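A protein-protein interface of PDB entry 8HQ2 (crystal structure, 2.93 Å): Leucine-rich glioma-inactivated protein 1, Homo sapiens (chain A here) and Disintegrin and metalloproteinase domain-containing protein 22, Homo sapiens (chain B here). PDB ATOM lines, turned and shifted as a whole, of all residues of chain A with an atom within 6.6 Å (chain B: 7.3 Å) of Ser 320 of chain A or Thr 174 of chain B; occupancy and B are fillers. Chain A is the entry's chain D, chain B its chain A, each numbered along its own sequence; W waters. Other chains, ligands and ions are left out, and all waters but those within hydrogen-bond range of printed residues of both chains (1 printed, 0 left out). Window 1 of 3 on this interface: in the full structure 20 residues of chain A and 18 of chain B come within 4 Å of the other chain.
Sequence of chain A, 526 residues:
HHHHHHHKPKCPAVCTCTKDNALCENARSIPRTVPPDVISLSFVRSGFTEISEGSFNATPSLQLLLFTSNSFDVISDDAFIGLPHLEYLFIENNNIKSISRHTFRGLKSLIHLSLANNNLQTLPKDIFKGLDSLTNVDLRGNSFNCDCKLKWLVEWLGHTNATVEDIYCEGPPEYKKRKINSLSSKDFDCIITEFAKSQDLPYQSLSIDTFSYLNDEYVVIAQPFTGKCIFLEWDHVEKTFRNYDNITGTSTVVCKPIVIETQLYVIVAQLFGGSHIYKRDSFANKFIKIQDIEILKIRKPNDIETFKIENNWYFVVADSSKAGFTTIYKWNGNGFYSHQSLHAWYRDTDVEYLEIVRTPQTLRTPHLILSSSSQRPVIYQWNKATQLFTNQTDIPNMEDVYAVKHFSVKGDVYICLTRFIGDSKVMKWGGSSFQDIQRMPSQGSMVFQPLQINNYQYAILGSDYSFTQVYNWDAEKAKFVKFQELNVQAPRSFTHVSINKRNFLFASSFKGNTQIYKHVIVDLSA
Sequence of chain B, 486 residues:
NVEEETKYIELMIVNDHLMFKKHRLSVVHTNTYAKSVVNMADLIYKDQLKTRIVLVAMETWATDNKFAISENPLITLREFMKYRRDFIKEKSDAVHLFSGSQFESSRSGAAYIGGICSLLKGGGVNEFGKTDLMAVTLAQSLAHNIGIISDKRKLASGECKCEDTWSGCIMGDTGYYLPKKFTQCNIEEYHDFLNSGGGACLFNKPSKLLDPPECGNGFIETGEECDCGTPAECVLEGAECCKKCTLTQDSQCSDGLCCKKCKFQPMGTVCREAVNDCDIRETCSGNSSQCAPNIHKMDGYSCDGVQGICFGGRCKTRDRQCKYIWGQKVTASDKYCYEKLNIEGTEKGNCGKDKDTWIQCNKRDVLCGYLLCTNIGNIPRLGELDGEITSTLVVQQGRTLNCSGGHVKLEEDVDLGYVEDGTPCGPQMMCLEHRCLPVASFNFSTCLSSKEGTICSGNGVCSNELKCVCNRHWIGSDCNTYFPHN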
ATOM      1  N   ARG A 299     -19.911  -6.380  32.992  1.00  0.00           N
ATOM      2  CA  ARG A 299     -19.151  -5.492  32.118  1.00  0.00           C
ATOM      3  C   ARG A 299     -19.703  -5.474  30.699  1.00  0.00           C
ATOM      4  O   ARG A 299     -20.103  -4.410  30.219  1.00  0.00           O
ATOM      5  CB  ARG A 299     -17.669  -5.890  32.126  1.00  0.00           C
ATOM      6  CG  ARG A 299     -17.062  -5.925  33.515  1.00  0.00           C
ATOM      7  CD  ARG A 299     -15.548  -5.895  33.468  1.00  0.00           C
ATOM      8  NE  ARG A 299     -14.977  -5.784  34.806  1.00  0.00           N
ATOM      9  CZ  ARG A 299     -13.720  -5.433  35.054  1.00  0.00           C
ATOM     10  NH1 ARG A 299     -12.897  -5.153  34.053  1.00  0.00           N
ATOM     11  NH2 ARG A 299     -13.286  -5.360  36.305  1.00  0.00           N
ATOM     12  N   LYS A 300     -19.713  -6.613  30.001  1.00  0.00           N
ATOM     13  CA  LYS A 300     -20.246  -6.715  28.643  1.00  0.00           C
ATOM     14  C   LYS A 300     -21.390  -7.728  28.639  1.00  0.00           C
ATOM     15  O   LYS A 300     -21.226  -8.863  28.164  1.00  0.00           O
ATOM     16  CB  LYS A 300     -19.152  -7.108  27.652  1.00  0.00           C
ATOM     17  CG  LYS A 300     -17.968  -6.157  27.617  1.00  0.00           C
ATOM     18  CD  LYS A 300     -18.350  -4.806  27.033  1.00  0.00           C
ATOM     19  CE  LYS A 300     -17.162  -3.853  27.000  1.00  0.00           C
ATOM     20  NZ  LYS A 300     -17.463  -2.638  26.194  1.00  0.00           N
ATOM     21  N   PRO A 301     -22.559  -7.357  29.163  1.00  0.00           N
ATOM     22  CA  PRO A 301     -23.663  -8.323  29.259  1.00  0.00           C
ATOM     23  C   PRO A 301     -24.209  -8.690  27.886  1.00  0.00           C
ATOM     24  O   PRO A 301     -24.531  -7.817  27.077  1.00  0.00           O
ATOM     25  CB  PRO A 301     -24.707  -7.580  30.098  1.00  0.00           C
ATOM     26  CG  PRO A 301     -24.442  -6.143  29.821  1.00  0.00           C
ATOM     27  CD  PRO A 301     -22.955  -6.019  29.635  1.00  0.00           C
ATOM     28  N   ASN A 302     -24.295  -9.994  27.619  1.00  0.00           N
ATOM     29  CA  ASN A 302     -24.916 -10.460  26.388  1.00  0.00           C
ATOM     30  C   ASN A 302     -26.360 -10.925  26.553  1.00  0.00           C
ATOM     31  O   ASN A 302     -27.067 -11.046  25.547  1.00  0.00           O
ATOM     32  CB  ASN A 302     -24.082 -11.602  25.787  1.00  0.00           C
ATOM     33  CG  ASN A 302     -24.381 -11.837  24.314  1.00  0.00           C
ATOM     34  OD1 ASN A 302     -24.851 -12.907  23.925  1.00  0.00           O
ATOM     35  ND2 ASN A 302     -24.125 -10.826  23.490  1.00  0.00           N
ATOM     36  N   ALA A 318     -25.641 -12.731  31.754  1.00  0.00           N
ATOM     37  CA  ALA A 318     -24.472 -13.371  31.170  1.00  0.00           C
ATOM     38  C   ALA A 318     -23.460 -12.306  30.779  1.00  0.00           C
ATOM     39  O   ALA A 318     -23.805 -11.336  30.098  1.00  0.00           O
ATOM     40  CB  ALA A 318     -24.857 -14.203  29.948  1.00  0.00           C
ATOM     41  N   ASP A 319     -22.217 -12.487  31.214  1.00  0.00           N
ATOM     42  CA  ASP A 319     -21.138 -11.545  30.945  1.00  0.00           C
ATOM     43  C   ASP A 319     -20.172 -12.213  29.975  1.00  0.00           C
ATOM     44  O   ASP A 319     -19.540 -13.219  30.315  1.00  0.00           O
ATOM     45  CB  ASP A 319     -20.437 -11.134  32.239  1.00  0.00           C
ATOM     46  CG  ASP A 319     -19.656  -9.835  32.100  1.00  0.00           C
ATOM     47  OD1 ASP A 319     -19.366  -9.424  30.958  1.00  0.00           O
ATOM     48  OD2 ASP A 319     -19.328  -9.224  33.141  1.00  0.00           O
ATOM     49  N   SER A 320     -20.067 -11.662  28.770  1.00  0.00           N
ATOM     50  CA  SER A 320     -19.167 -12.189  27.754  1.00  0.00           C
ATOM     51  C   SER A 320     -17.749 -11.642  27.874  1.00  0.00           C
ATOM     52  O   SER A 320     -16.899 -11.977  27.044  1.00  0.00           O
ATOM     53  CB  SER A 320     -19.725 -11.897  26.358  1.00  0.00           C
ATOM     54  OG  SER A 320     -20.094 -10.535  26.235  1.00  0.00           O
ATOM     55  N   SER A 321     -17.477 -10.789  28.856  1.00  0.00           N
ATOM     56  CA  SER A 321     -16.123 -10.339  29.137  1.00  0.00           C
ATOM     57  C   SER A 321     -15.415 -11.313  30.071  1.00  0.00           C
ATOM     58  O   SER A 321     -16.033 -11.928  30.945  1.00  0.00           O
ATOM     59  CB  SER A 321     -16.130  -8.941  29.753  1.00  0.00           C
ATOM     60  OG  SER A 321     -16.761  -8.954  31.017  1.00  0.00           O
ATOM     61  N   LYS A 322     -14.099 -11.447  29.874  1.00  0.00           N
ATOM     62  CA  LYS A 322     -13.292 -12.294  30.748  1.00  0.00           C
ATOM     63  C   LYS A 322     -13.221 -11.738  32.168  1.00  0.00           C
ATOM     64  O   LYS A 322     -13.187 -12.512  33.133  1.00  0.00           O
ATOM     65  CB  LYS A 322     -11.885 -12.452  30.162  1.00  0.00           C
ATOM     66  CG  LYS A 322     -10.857 -13.046  31.114  1.00  0.00           C
ATOM     67  CD  LYS A 322     -11.107 -14.522  31.366  1.00  0.00           C
ATOM     68  CE  LYS A 322     -10.410 -15.386  30.340  1.00  0.00           C
ATOM     69  NZ  LYS A 322      -9.365 -16.205  30.992  1.00  0.00           N
ATOM     70  N   ALA A 323     -13.221 -10.409  32.317  1.00  0.00           N
ATOM     71  CA  ALA A 323     -13.095  -9.799  33.638  1.00  0.00           C
ATOM     72  C   ALA A 323     -14.379  -9.905  34.456  1.00  0.00           C
ATOM     73  O   ALA A 323     -14.331 -10.231  35.646  1.00  0.00           O
ATOM     74  CB  ALA A 323     -12.678  -8.333  33.498  1.00  0.00           C
ATOM     75  N   GLY A 324     -15.531  -9.619  33.848  1.00  0.00           N
ATOM     76  CA  GLY A 324     -16.782  -9.704  34.569  1.00  0.00           C
ATOM     77  C   GLY A 324     -17.255 -11.136  34.766  1.00  0.00           C
ATOM     78  O   GLY A 324     -16.788 -12.068  34.114  1.00  0.00           O
ATOM     79  N   THR A 326     -20.727 -13.759  35.333  1.00  0.00           N
ATOM     80  CA  THR A 326     -22.164 -13.982  35.248  1.00  0.00           C
ATOM     81  C   THR A 326     -22.748 -14.114  36.649  1.00  0.00           C
ATOM     82  O   THR A 326     -22.273 -14.918  37.456  1.00  0.00           O
ATOM     83  CB  THR A 326     -22.452 -15.236  34.421  1.00  0.00           C
ATOM     84  OG1 THR A 326     -22.242 -14.955  33.031  1.00  0.00           O
ATOM     85  CG2 THR A 326     -23.882 -15.708  34.632  1.00  0.00           C
ATOM     86  N   TYR A 346     -14.897 -16.941  32.079  1.00  0.00           N
ATOM     87  CA  TYR A 346     -15.367 -17.402  30.784  1.00  0.00           C
ATOM     88  C   TYR A 346     -16.186 -16.301  30.128  1.00  0.00           C
ATOM     89  O   TYR A 346     -16.679 -15.386  30.792  1.00  0.00           O
ATOM     90  CB  TYR A 346     -16.216 -18.671  30.902  1.00  0.00           C
ATOM     91  CG  TYR A 346     -15.444 -19.919  31.260  1.00  0.00           C
ATOM     92  CD1 TYR A 346     -15.137 -20.212  32.580  1.00  0.00           C
ATOM     93  CD2 TYR A 346     -15.034 -20.809  30.277  1.00  0.00           C
ATOM     94  CE1 TYR A 346     -14.432 -21.354  32.913  1.00  0.00           C
ATOM     95  CE2 TYR A 346     -14.330 -21.953  30.599  1.00  0.00           C
ATOM     96  CZ  TYR A 346     -14.032 -22.220  31.918  1.00  0.00           C
ATOM     97  OH  TYR A 346     -13.330 -23.357  32.246  1.00  0.00           O
ATOM     98  N   ARG A 347     -16.332 -16.396  28.810  1.00  0.00           N
ATOM     99  CA  ARG A 347     -17.116 -15.434  28.045  1.00  0.00           C
ATOM    100  C   ARG A 347     -18.498 -16.036  27.835  1.00  0.00           C
ATOM    101  O   ARG A 347     -18.659 -16.968  27.044  1.00  0.00           O
ATOM    102  CB  ARG A 347     -16.428 -15.111  26.722  1.00  0.00           C
ATOM    103  CG  ARG A 347     -15.007 -14.605  26.901  1.00  0.00           C
ATOM    104  CD  ARG A 347     -14.445 -13.990  25.632  1.00  0.00           C
ATOM    105  NE  ARG A 347     -13.418 -12.992  25.931  1.00  0.00           N
ATOM    106  CZ  ARG A 347     -12.135 -13.273  26.132  1.00  0.00           C
ATOM    107  NH1 ARG A 347     -11.706 -14.527  26.068  1.00  0.00           N
ATOM    108  NH2 ARG A 347     -11.277 -12.297  26.399  1.00  0.00           N
ATOM    109  N   ASP A 348     -19.498 -15.489  28.520  1.00  0.00           N
ATOM    110  CA  ASP A 348     -20.831 -16.080  28.563  1.00  0.00           C
ATOM    111  C   ASP A 348     -21.736 -15.361  27.568  1.00  0.00           C
ATOM    112  O   ASP A 348     -22.035 -14.174  27.730  1.00  0.00           O
ATOM    113  CB  ASP A 348     -21.401 -16.017  29.977  1.00  0.00           C
ATOM    114  CG  ASP A 348     -20.635 -16.892  30.948  1.00  0.00           C
ATOM    115  OD1 ASP A 348     -19.905 -17.794  30.482  1.00  0.00           O
ATOM    116  OD2 ASP A 348     -20.762 -16.683  32.172  1.00  0.00           O
ATOM    117  N   THR A 349     -22.154 -16.082  26.527  1.00  0.00           N
ATOM    118  CA  THR A 349     -23.049 -15.513  25.528  1.00  0.00           C
ATOM    119  C   THR A 349     -24.519 -15.571  25.934  1.00  0.00           C
ATOM    120  O   THR A 349     -25.283 -14.667  25.577  1.00  0.00           O
ATOM    121  CB  THR A 349     -22.850 -16.218  24.187  1.00  0.00           C
ATOM    122  OG1 THR A 349     -22.672 -17.624  24.397  1.00  0.00           O
ATOM    123  CG2 THR A 349     -21.632 -15.655  23.481  1.00  0.00           C
ATOM    124  N   SER A 373     -18.365 -18.860  25.028  1.00  0.00           N
ATOM    125  CA  SER A 373     -17.797 -18.831  23.688  1.00  0.00           C
ATOM    126  C   SER A 373     -16.574 -19.738  23.614  1.00  0.00           C
ATOM    127  O   SER A 373     -15.747 -19.765  24.528  1.00  0.00           O
ATOM    128  CB  SER A 373     -17.416 -17.406  23.297  1.00  0.00           C
ATOM    129  OG  SER A 373     -16.083 -17.123  23.678  1.00  0.00           O
ATOM    130  N   SER B 108      -6.738 -12.132  29.537  1.00  0.00           N
ATOM    131  CA  SER B 108      -6.694 -13.237  28.589  1.00  0.00           C
ATOM    132  C   SER B 108      -5.286 -13.472  28.067  1.00  0.00           C
ATOM    133  O   SER B 108      -5.081 -14.375  27.248  1.00  0.00           O
ATOM    134  CB  SER B 108      -7.647 -12.982  27.415  1.00  0.00           C
ATOM    135  OG  SER B 108      -7.344 -11.766  26.751  1.00  0.00           O
ATOM    136  N   LEU B 133     -11.038 -13.577  18.287  1.00  0.00           N
ATOM    137  CA  LEU B 133     -10.660 -13.299  19.671  1.00  0.00           C
ATOM    138  C   LEU B 133      -9.153 -13.419  19.869  1.00  0.00           C
ATOM    139  O   LEU B 133      -8.544 -12.583  20.545  1.00  0.00           O
ATOM    140  CB  LEU B 133     -11.402 -14.239  20.623  1.00  0.00           C
ATOM    141  CG  LEU B 133     -11.158 -13.959  22.108  1.00  0.00           C
ATOM    142  CD1 LEU B 133     -11.782 -12.633  22.494  1.00  0.00           C
ATOM    143  CD2 LEU B 133     -11.702 -15.065  22.986  1.00  0.00           C
ATOM    144  N   VAL B 136      -7.396 -10.298  18.562  1.00  0.00           N
ATOM    145  CA  VAL B 136      -7.452  -9.169  19.487  1.00  0.00           C
ATOM    146  C   VAL B 136      -6.527  -9.407  20.675  1.00  0.00           C
ATOM    147  O   VAL B 136      -5.840  -8.490  21.139  1.00  0.00           O
ATOM    148  CB  VAL B 136      -8.901  -8.914  19.938  1.00  0.00           C
ATOM    149  CG1 VAL B 136      -8.939  -7.907  21.077  1.00  0.00           C
ATOM    150  CG2 VAL B 136      -9.734  -8.427  18.771  1.00  0.00           C
ATOM    151  N   THR B 137      -6.500 -10.639  21.190  1.00  0.00           N
ATOM    152  CA  THR B 137      -5.611 -10.970  22.301  1.00  0.00           C
ATOM    153  C   THR B 137      -4.152 -10.767  21.909  1.00  0.00           C
ATOM    154  O   THR B 137      -3.363 -10.199  22.674  1.00  0.00           O
ATOM    155  CB  THR B 137      -5.851 -12.407  22.758  1.00  0.00           C
ATOM    156  OG1 THR B 137      -7.199 -12.541  23.226  1.00  0.00           O
ATOM    157  CG2 THR B 137      -4.888 -12.783  23.877  1.00  0.00           C
ATOM    158  N   GLN B 140      -3.422  -6.937  21.752  1.00  0.00           N
ATOM    159  CA  GLN B 140      -3.197  -6.230  23.007  1.00  0.00           C
ATOM    160  C   GLN B 140      -1.913  -6.677  23.693  1.00  0.00           C
ATOM    161  O   GLN B 140      -1.270  -5.870  24.371  1.00  0.00           O
ATOM    162  CB  GLN B 140      -4.390  -6.413  23.950  1.00  0.00           C
ATOM    163  CG  GLN B 140      -4.834  -7.849  24.147  1.00  0.00           C
ATOM    164  CD  GLN B 140      -6.162  -7.960  24.872  1.00  0.00           C
ATOM    165  OE1 GLN B 140      -7.080  -7.170  24.645  1.00  0.00           O
ATOM    166  NE2 GLN B 140      -6.264  -8.941  25.763  1.00  0.00           N
ATOM    167  N   GLY B 168     -15.664  -1.982  22.388  1.00  0.00           N
ATOM    168  CA  GLY B 168     -14.597  -1.211  22.992  1.00  0.00           C
ATOM    169  C   GLY B 168     -13.454  -0.945  22.034  1.00  0.00           C
ATOM    170  O   GLY B 168     -13.629  -1.045  20.815  1.00  0.00           O
ATOM    171  N   CYS B 169     -12.309  -0.543  22.565  1.00  0.00           N
ATOM    172  CA  CYS B 169     -11.066  -0.555  21.812  1.00  0.00           C
ATOM    173  C   CYS B 169     -10.269  -1.798  22.210  1.00  0.00           C
ATOM    174  O   CYS B 169     -10.700  -2.586  23.053  1.00  0.00           O
ATOM    175  CB  CYS B 169     -10.283   0.742  22.037  1.00  0.00           C
ATOM    176  SG  CYS B 169     -10.988   2.182  21.170  1.00  0.00           S
ATOM    177  N   ILE B 170      -9.100  -1.985  21.588  1.00  0.00           N
ATOM    178  CA  ILE B 170      -8.359  -3.230  21.789  1.00  0.00           C
ATOM    179  C   ILE B 170      -7.943  -3.387  23.247  1.00  0.00           C
ATOM    180  O   ILE B 170      -8.085  -4.466  23.837  1.00  0.00           O
ATOM    181  CB  ILE B 170      -7.142  -3.296  20.847  1.00  0.00           C
ATOM    182  CG1 ILE B 170      -7.558  -3.757  19.452  1.00  0.00           C
ATOM    183  CG2 ILE B 170      -6.093  -4.249  21.393  1.00  0.00           C
ATOM    184  CD1 ILE B 170      -8.034  -2.655  18.556  1.00  0.00           C
ATOM    185  N   MET B 171      -7.431  -2.317  23.856  1.00  0.00           N
ATOM    186  CA  MET B 171      -6.868  -2.430  25.196  1.00  0.00           C
ATOM    187  C   MET B 171      -7.926  -2.644  26.270  1.00  0.00           C
ATOM    188  O   MET B 171      -7.586  -3.094  27.371  1.00  0.00           O
ATOM    189  CB  MET B 171      -6.042  -1.186  25.521  1.00  0.00           C
ATOM    190  CG  MET B 171      -4.895  -0.943  24.548  1.00  0.00           C
ATOM    191  SD  MET B 171      -4.127  -2.475  23.998  1.00  0.00           S
ATOM    192  CE  MET B 171      -3.234  -2.956  25.475  1.00  0.00           C
ATOM    193  N   GLY B 172      -9.193  -2.354  25.980  1.00  0.00           N
ATOM    194  CA  GLY B 172     -10.251  -2.494  26.959  1.00  0.00           C
ATOM    195  C   GLY B 172     -10.705  -3.928  27.149  1.00  0.00           C
ATOM    196  O   GLY B 172     -10.202  -4.868  26.536  1.00  0.00           O
ATOM    197  N   ASP B 173     -11.676  -4.091  28.046  1.00  0.00           N
ATOM    198  CA  ASP B 173     -12.298  -5.395  28.246  1.00  0.00           C
ATOM    199  C   ASP B 173     -13.036  -5.820  26.983  1.00  0.00           C
ATOM    200  O   ASP B 173     -13.786  -5.036  26.393  1.00  0.00           O
ATOM    201  CB  ASP B 173     -13.265  -5.354  29.430  1.00  0.00           C
ATOM    202  CG  ASP B 173     -12.603  -4.882  30.709  1.00  0.00           C
ATOM    203  OD1 ASP B 173     -11.402  -5.166  30.904  1.00  0.00           O
ATOM    204  OD2 ASP B 173     -13.292  -4.235  31.528  1.00  0.00           O
ATOM    205  N   THR B 174     -12.825  -7.067  26.571  1.00  0.00           N
ATOM    206  CA  THR B 174     -13.382  -7.590  25.332  1.00  0.00           C
ATOM    207  C   THR B 174     -14.630  -8.408  25.640  1.00  0.00           C
ATOM    208  O   THR B 174     -14.556  -9.416  26.350  1.00  0.00           O
ATOM    209  CB  THR B 174     -12.359  -8.449  24.588  1.00  0.00           C
ATOM    210  OG1 THR B 174     -11.955  -9.539  25.426  1.00  0.00           O
ATOM    211  CG2 THR B 174     -11.138  -7.625  24.218  1.00  0.00           C
ATOM    212  N   GLY B 175     -15.768  -7.966  25.113  1.00  0.00           N
ATOM    213  CA  GLY B 175     -17.006  -8.710  25.192  1.00  0.00           C
ATOM    214  C   GLY B 175     -17.214  -9.562  23.958  1.00  0.00           C
ATOM    215  O   GLY B 175     -16.276  -9.878  23.221  1.00  0.00           O
ATOM    216  N   TYR B 176     -18.476  -9.934  23.725  1.00  0.00           N
ATOM    217  CA  TYR B 176     -18.787 -10.726  22.540  1.00  0.00           C
ATOM    218  C   TYR B 176     -18.549  -9.945  21.254  1.00  0.00           C
ATOM    219  O   TYR B 176     -18.182 -10.537  20.231  1.00  0.00           O
ATOM    220  CB  TYR B 176     -20.232 -11.227  22.584  1.00  0.00           C
ATOM    221  CG  TYR B 176     -20.631 -11.926  21.306  1.00  0.00           C
ATOM    222  CD1 TYR B 176     -20.193 -13.216  21.034  1.00  0.00           C
ATOM    223  CD2 TYR B 176     -21.416 -11.286  20.356  1.00  0.00           C
ATOM    224  CE1 TYR B 176     -20.540 -13.854  19.861  1.00  0.00           C
ATOM    225  CE2 TYR B 176     -21.766 -11.918  19.178  1.00  0.00           C
ATOM    226  CZ  TYR B 176     -21.325 -13.202  18.937  1.00  0.00           C
ATOM    227  OH  TYR B 176     -21.670 -13.837  17.768  1.00  0.00           O
ATOM    228  N   TYR B 177     -18.778  -8.637  21.273  1.00  0.00           N
ATOM    229  CA  TYR B 177     -18.537  -7.789  20.112  1.00  0.00           C
ATOM    230  C   TYR B 177     -17.109  -7.256  20.185  1.00  0.00           C
ATOM    231  O   TYR B 177     -16.747  -6.560  21.140  1.00  0.00           O
ATOM    232  CB  TYR B 177     -19.554  -6.651  20.059  1.00  0.00           C
ATOM    233  CG  TYR B 177     -20.988  -7.131  19.974  1.00  0.00           C
ATOM    234  CD1 TYR B 177     -21.557  -7.479  18.755  1.00  0.00           C
ATOM    235  CD2 TYR B 177     -21.773  -7.239  21.117  1.00  0.00           C
ATOM    236  CE1 TYR B 177     -22.866  -7.915  18.677  1.00  0.00           C
ATOM    237  CE2 TYR B 177     -23.084  -7.676  21.047  1.00  0.00           C
ATOM    238  CZ  TYR B 177     -23.624  -8.012  19.825  1.00  0.00           C
ATOM    239  OH  TYR B 177     -24.928  -8.448  19.751  1.00  0.00           O
ATOM    240  N   LEU B 178     -16.290  -7.594  19.167  1.00  0.00           N
ATOM    241  CA  LEU B 178     -14.845  -7.418  19.238  1.00  0.00           C
ATOM    242  C   LEU B 178     -14.421  -6.055  18.700  1.00  0.00           C
ATOM    243  O   LEU B 178     -14.987  -5.571  17.713  1.00  0.00           O
ATOM    244  CB  LEU B 178     -14.139  -8.522  18.456  1.00  0.00           C
ATOM    245  CG  LEU B 178     -14.417  -9.910  19.028  1.00  0.00           C
ATOM    246  CD1 LEU B 178     -13.622 -10.954  18.289  1.00  0.00           C
ATOM    247  CD2 LEU B 178     -14.103  -9.948  20.516  1.00  0.00           C
ATOM    248  N   PRO B 179     -13.454  -5.424  19.367  1.00  0.00           N
ATOM    249  CA  PRO B 179     -12.909  -4.149  18.881  1.00  0.00           C
ATOM    250  C   PRO B 179     -11.953  -4.330  17.711  1.00  0.00           C
ATOM    251  O   PRO B 179     -11.156  -5.270  17.677  1.00  0.00           O
ATOM    252  CB  PRO B 179     -12.176  -3.602  20.108  1.00  0.00           C
ATOM    253  CG  PRO B 179     -11.764  -4.821  20.863  1.00  0.00           C
ATOM    254  CD  PRO B 179     -12.833  -5.853  20.633  1.00  0.00           C
HETATM  255  O   HOH W   1     -26.010  -9.800  21.818  1.00  0.00           O
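Asp 173 of chain B touches Lys 300 of chain A (O to CE, 3.6 Å).
Lys 300 of chain A touches Gly 175 of chain B.
O of Ser 320 of chain A touches O of Thr 174 of chain B, 3.5 Å away.
OG of Ser 320 of chain A touches CA of Gly 175 of chain B (3.7 Å).
O of Thr 174 of chain B touches CA of Ser 321 of chain A, 3.3 Å away.
CB of Ser 108 of chain B touches NH2 of Arg 347 of chain A, 3.8 Å away.
Leu 133 of chain B touches Arg 347 of chain A.
Thr 349 of chain A touches Tyr 176 of chain B (CG2 to CD1, 3.7 Å).
Water W1 lies within hydrogen-bond range of the side-chain hydroxyl (OH) of Tyr 177 of chain B (2.7 Å) and the side-chain amide nitrogen (ND2) of Asn 302 of chain A (2.7 Å).
Of the 17 printed residues of chain B, 6 touch a printed residue of chain A.
Hydrophobic or aromatic side chains of chain B that line the printed part of chain A: Leu 133 and Tyr 176.
Among the printed residues, 11 pairs touch across the chains.
Among the printed residues, Asp or Glu carboxylates within 4 Å of a Lys or Arg side-chain nitrogen of the other chain: Arg 299 of chain A with Asp 173 of chain B (2.7 Å).
The guanidinium group of Arg 347 of chain A lies within hydrogen-bond range of the side-chain hydroxyl of Thr 174 of chain B (3.0 Å).
The guanidinium group (NH1) of Arg 299 of chain A is in salt-bridge range of the side-chain carboxylate (OD2) of Asp 173 of chain B (2.7 Å).
N of Tyr 176 of chain B sits at hydrogen-bond distance from OG of Ser 320 of chain A, at 3.0 Å.
Ser 320 of chain A touches just these residues of chain B: Thr 174 (3.5 Å), Gly 175 (3.7 Å) and Tyr 176 (3.0 Å).
Of the printed residues of chain A, Asp 173 of chain B touches Arg 299 and Lys 300.
Of the printed residues of chain B, Arg 299 of chain A touches Asp 173 (2.7 Å).
Printed residues of chain B within 4 Å of Thr 349 of chain A: Tyr 176 (3.7 Å).
Of the printed residues of chain A, Ser 108 of chain B touches Arg 347 (3.8 Å).
Cys 169 of chain B touches none of the printed residues of chain A.
The nearest residue of chain A that does not touch Thr 174 of chain B is Lys 322 of chain A (4.1 Å).
N of Gly 324 of chain A lies within hydrogen-bond range of OG of Ser 321 of chain A.
OG of Ser 321 of chain A is in hydrogen-bond range of OD1 of Asp 319 of chain A (2.6 Å).
The backbone carbonyl oxygen (O) of Lys 300 of chain A is in hydrogen-bond range of the side-chain hydroxyl (OG) of Ser 320 of chain A, 2.8 Å away.
OG of Ser 108 of chain B is in hydrogen-bond range of NE2 of Gln 140 of chain B (3.2 Å).
The side-chain amide oxygen of Asn 302 of chain A sits close to the backbone carbonyl oxygen of Thr 349 of chain A, 2.5 Å away.
The side-chain carboxylate of Asp 319 of chain A is in hydrogen-bond range of the backbone NH of Arg 299 of chain A, 2.9 Å away.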
